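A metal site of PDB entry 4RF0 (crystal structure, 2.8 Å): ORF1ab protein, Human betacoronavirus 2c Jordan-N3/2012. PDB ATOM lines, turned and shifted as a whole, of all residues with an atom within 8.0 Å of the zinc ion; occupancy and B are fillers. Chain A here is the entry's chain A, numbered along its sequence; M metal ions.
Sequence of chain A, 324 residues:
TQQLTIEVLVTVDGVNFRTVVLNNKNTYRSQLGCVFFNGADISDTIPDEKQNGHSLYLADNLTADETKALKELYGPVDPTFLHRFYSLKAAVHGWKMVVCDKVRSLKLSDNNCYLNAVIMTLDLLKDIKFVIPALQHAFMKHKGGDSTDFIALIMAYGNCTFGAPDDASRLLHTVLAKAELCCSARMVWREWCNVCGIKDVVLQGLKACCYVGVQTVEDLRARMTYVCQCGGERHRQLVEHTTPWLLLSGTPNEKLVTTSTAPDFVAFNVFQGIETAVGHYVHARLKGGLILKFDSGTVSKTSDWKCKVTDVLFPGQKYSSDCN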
ATOM      1  N   TRP A 192      -1.880 -19.020   7.516  1.00  0.00           N
ATOM      2  CA  TRP A 192      -0.752 -19.173   8.421  1.00  0.00           C
ATOM      3  C   TRP A 192       0.487 -18.402   7.981  1.00  0.00           C
ATOM      4  O   TRP A 192       0.775 -18.277   6.792  1.00  0.00           O
ATOM      5  CB  TRP A 192      -0.402 -20.659   8.606  1.00  0.00           C
ATOM      6  CG  TRP A 192       0.229 -21.305   7.406  1.00  0.00           C
ATOM      7  CD1 TRP A 192       1.559 -21.366   7.118  1.00  0.00           C
ATOM      8  CD2 TRP A 192      -0.444 -22.010   6.359  1.00  0.00           C
ATOM      9  NE1 TRP A 192       1.758 -22.052   5.946  1.00  0.00           N
ATOM     10  CE2 TRP A 192       0.551 -22.461   5.467  1.00  0.00           C
ATOM     11  CE3 TRP A 192      -1.784 -22.300   6.095  1.00  0.00           C
ATOM     12  CZ2 TRP A 192       0.231 -23.191   4.312  1.00  0.00           C
ATOM     13  CZ3 TRP A 192      -2.093 -23.019   4.947  1.00  0.00           C
ATOM     14  CH2 TRP A 192      -1.082 -23.455   4.076  1.00  0.00           C
ATOM     15  N   CYS A 193       1.198 -17.879   8.977  1.00  0.00           N
ATOM     16  CA  CYS A 193       2.430 -17.141   8.771  1.00  0.00           C
ATOM     17  C   CYS A 193       3.459 -17.636   9.781  1.00  0.00           C
ATOM     18  O   CYS A 193       3.155 -17.743  10.965  1.00  0.00           O
ATOM     19  CB  CYS A 193       2.198 -15.638   8.914  1.00  0.00           C
ATOM     20  SG  CYS A 193       3.671 -14.645   9.250  1.00  0.00           S
ATOM     21  N   ASN A 194       4.661 -17.942   9.307  1.00  0.00           N
ATOM     22  CA  ASN A 194       5.716 -18.494  10.164  1.00  0.00           C
ATOM     23  C   ASN A 194       6.037 -17.615  11.368  1.00  0.00           C
ATOM     24  O   ASN A 194       6.546 -18.097  12.379  1.00  0.00           O
ATOM     25  CB  ASN A 194       6.989 -18.736   9.342  1.00  0.00           C
ATOM     26  CG  ASN A 194       6.863 -19.915   8.408  1.00  0.00           C
ATOM     27  OD1 ASN A 194       6.194 -20.903   8.715  1.00  0.00           O
ATOM     28  ND2 ASN A 194       7.514 -19.830   7.248  1.00  0.00           N
ATOM     29  N   VAL A 195       5.727 -16.330  11.259  1.00  0.00           N
ATOM     30  CA  VAL A 195       6.010 -15.372  12.321  1.00  0.00           C
ATOM     31  C   VAL A 195       4.788 -15.104  13.192  1.00  0.00           C
ATOM     32  O   VAL A 195       4.865 -15.192  14.421  1.00  0.00           O
ATOM     33  CB  VAL A 195       6.508 -14.035  11.743  1.00  0.00           C
ATOM     34  CG1 VAL A 195       6.687 -13.003  12.846  1.00  0.00           C
ATOM     35  CG2 VAL A 195       7.809 -14.237  10.977  1.00  0.00           C
ATOM     36  N   CYS A 196       3.669 -14.783  12.563  1.00  0.00           N
ATOM     37  CA  CYS A 196       2.473 -14.369  13.290  1.00  0.00           C
ATOM     38  C   CYS A 196       1.678 -15.539  13.859  1.00  0.00           C
ATOM     39  O   CYS A 196       1.209 -15.477  14.999  1.00  0.00           O
ATOM     40  CB  CYS A 196       1.570 -13.525  12.381  1.00  0.00           C
ATOM     41  SG  CYS A 196       2.378 -12.033  11.732  1.00  0.00           S
ATOM     42  N   GLY A 197       1.524 -16.603  13.089  1.00  0.00           N
ATOM     43  CA  GLY A 197       0.849 -17.798  13.562  1.00  0.00           C
ATOM     44  C   GLY A 197      -0.218 -18.344  12.632  1.00  0.00           C
ATOM     45  O   GLY A 197      -0.453 -17.814  11.549  1.00  0.00           O
ATOM     46  N   VAL A 227       0.920 -11.547   1.023  1.00  0.00           N
ATOM     47  CA  VAL A 227       1.714 -10.832   2.014  1.00  0.00           C
ATOM     48  C   VAL A 227       0.970 -10.648   3.334  1.00  0.00           C
ATOM     49  O   VAL A 227      -0.165 -10.170   3.358  1.00  0.00           O
ATOM     50  CB  VAL A 227       2.156  -9.456   1.479  1.00  0.00           C
ATOM     51  CG1 VAL A 227       3.051  -8.757   2.487  1.00  0.00           C
ATOM     52  CG2 VAL A 227       2.867  -9.603   0.148  1.00  0.00           C
ATOM     53  N   CYS A 228       1.611 -11.027   4.429  1.00  0.00           N
ATOM     54  CA  CYS A 228       1.055 -10.845   5.760  1.00  0.00           C
ATOM     55  C   CYS A 228       1.133  -9.384   6.182  1.00  0.00           C
ATOM     56  O   CYS A 228       1.811  -8.584   5.530  1.00  0.00           O
ATOM     57  CB  CYS A 228       1.795 -11.722   6.779  1.00  0.00           C
ATOM     58  SG  CYS A 228       1.198 -11.583   8.479  1.00  0.00           S
ATOM     59  N   GLN A 229       0.436  -9.035   7.253  1.00  0.00           N
ATOM     60  CA  GLN A 229       0.407  -7.647   7.716  1.00  0.00           C
ATOM     61  C   GLN A 229       1.765  -7.192   8.236  1.00  0.00           C
ATOM     62  O   GLN A 229       2.049  -5.993   8.289  1.00  0.00           O
ATOM     63  CB  GLN A 229      -0.653  -7.473   8.817  1.00  0.00           C
ATOM     64  CG  GLN A 229      -2.054  -7.868   8.392  1.00  0.00           C
ATOM     65  CD  GLN A 229      -3.101  -7.437   9.407  1.00  0.00           C
ATOM     66  OE1 GLN A 229      -2.840  -6.600  10.268  1.00  0.00           O
ATOM     67  NE2 GLN A 229      -4.300  -8.012   9.297  1.00  0.00           N
ATOM     68  N   CYS A 230       2.609  -8.147   8.626  1.00  0.00           N
ATOM     69  CA  CYS A 230       3.932  -7.836   9.146  1.00  0.00           C
ATOM     70  C   CYS A 230       4.930  -7.575   8.014  1.00  0.00           C
ATOM     71  O   CYS A 230       5.978  -6.976   8.235  1.00  0.00           O
ATOM     72  CB  CYS A 230       4.432  -8.970  10.040  1.00  0.00           C
ATOM     73  SG  CYS A 230       4.417 -10.601   9.265  1.00  0.00           S
ATOM     74  N   GLY A 231       4.585  -8.032   6.812  1.00  0.00           N
ATOM     75  CA  GLY A 231       5.430  -7.830   5.659  1.00  0.00           C
ATOM     76  C   GLY A 231       5.993  -9.125   5.101  1.00  0.00           C
ATOM     77  O   GLY A 231       6.504  -9.161   3.981  1.00  0.00           O
ATOM     78  N   GLY A 232       5.898 -10.190   5.895  1.00  0.00           N
ATOM     79  CA  GLY A 232       6.441 -11.476   5.500  1.00  0.00           C
ATOM     80  C   GLY A 232       5.492 -12.308   4.654  1.00  0.00           C
ATOM     81  O   GLY A 232       4.349 -11.932   4.432  1.00  0.00           O
ATOM     82  N   GLU A 233       5.978 -13.456   4.209  1.00  0.00           N
ATOM     83  CA  GLU A 233       5.192 -14.371   3.384  1.00  0.00           C
ATOM     84  C   GLU A 233       4.030 -14.951   4.182  1.00  0.00           C
ATOM     85  O   GLU A 233       4.220 -15.469   5.293  1.00  0.00           O
ATOM     86  CB  GLU A 233       6.069 -15.489   2.828  1.00  0.00           C
ATOM     87  CG  GLU A 233       5.365 -16.428   1.871  1.00  0.00           C
ATOM     88  CD  GLU A 233       6.308 -17.453   1.247  1.00  0.00           C
ATOM     89  OE1 GLU A 233       7.456 -17.569   1.730  1.00  0.00           O
ATOM     90  OE2 GLU A 233       5.905 -18.119   0.272  1.00  0.00           O
ATOM     91  N   ARG A 234       2.832 -14.862   3.626  1.00  0.00           N
ATOM     92  CA  ARG A 234       1.640 -15.431   4.255  1.00  0.00           C
ATOM     93  C   ARG A 234       1.000 -16.441   3.317  1.00  0.00           C
ATOM     94  O   ARG A 234       1.078 -16.300   2.100  1.00  0.00           O
ATOM     95  CB  ARG A 234       0.639 -14.333   4.635  1.00  0.00           C
ATOM     96  CG  ARG A 234      -0.523 -14.829   5.475  1.00  0.00           C
ATOM     97  CD  ARG A 234      -1.351 -13.683   6.015  1.00  0.00           C
ATOM     98  NE  ARG A 234      -2.386 -14.135   6.941  1.00  0.00           N
ATOM     99  CZ  ARG A 234      -2.200 -14.271   8.251  1.00  0.00           C
ATOM    100  NH1 ARG A 234      -1.014 -13.984   8.782  1.00  0.00           N
ATOM    101  NH2 ARG A 234      -3.179 -14.709   9.021  1.00  0.00           N
HETATM  102 ZN    ZN M   1       3.050 -12.437   9.560  1.00  0.00          ZN
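The side-chain sulfur (SG) of Cys 230 sits close to the backbone NH (N) of Gly 232 (3.7 Å).
The side-chain sulfur (SG) of Cys 228 sits close to the guanidinium group (NH1) of Arg 234 (3.3 Å).
N of Val 195 lies close to SG of Cys 193.
Of the 14 residues printed, 4 come within 4 Å of the zinc ion.
Along chain A the residues within 4 Å of the zinc ion span positions 193 to 230.
The zinc ion is bound by the side-chain sulfur of Cys 230 (2.3 Å), the side-chain sulfur of Cys 228 (2.3 Å), the side-chain sulfur of Cys 196 (2.3 Å) and the side-chain sulfur of Cys 193 (2.3 Å).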
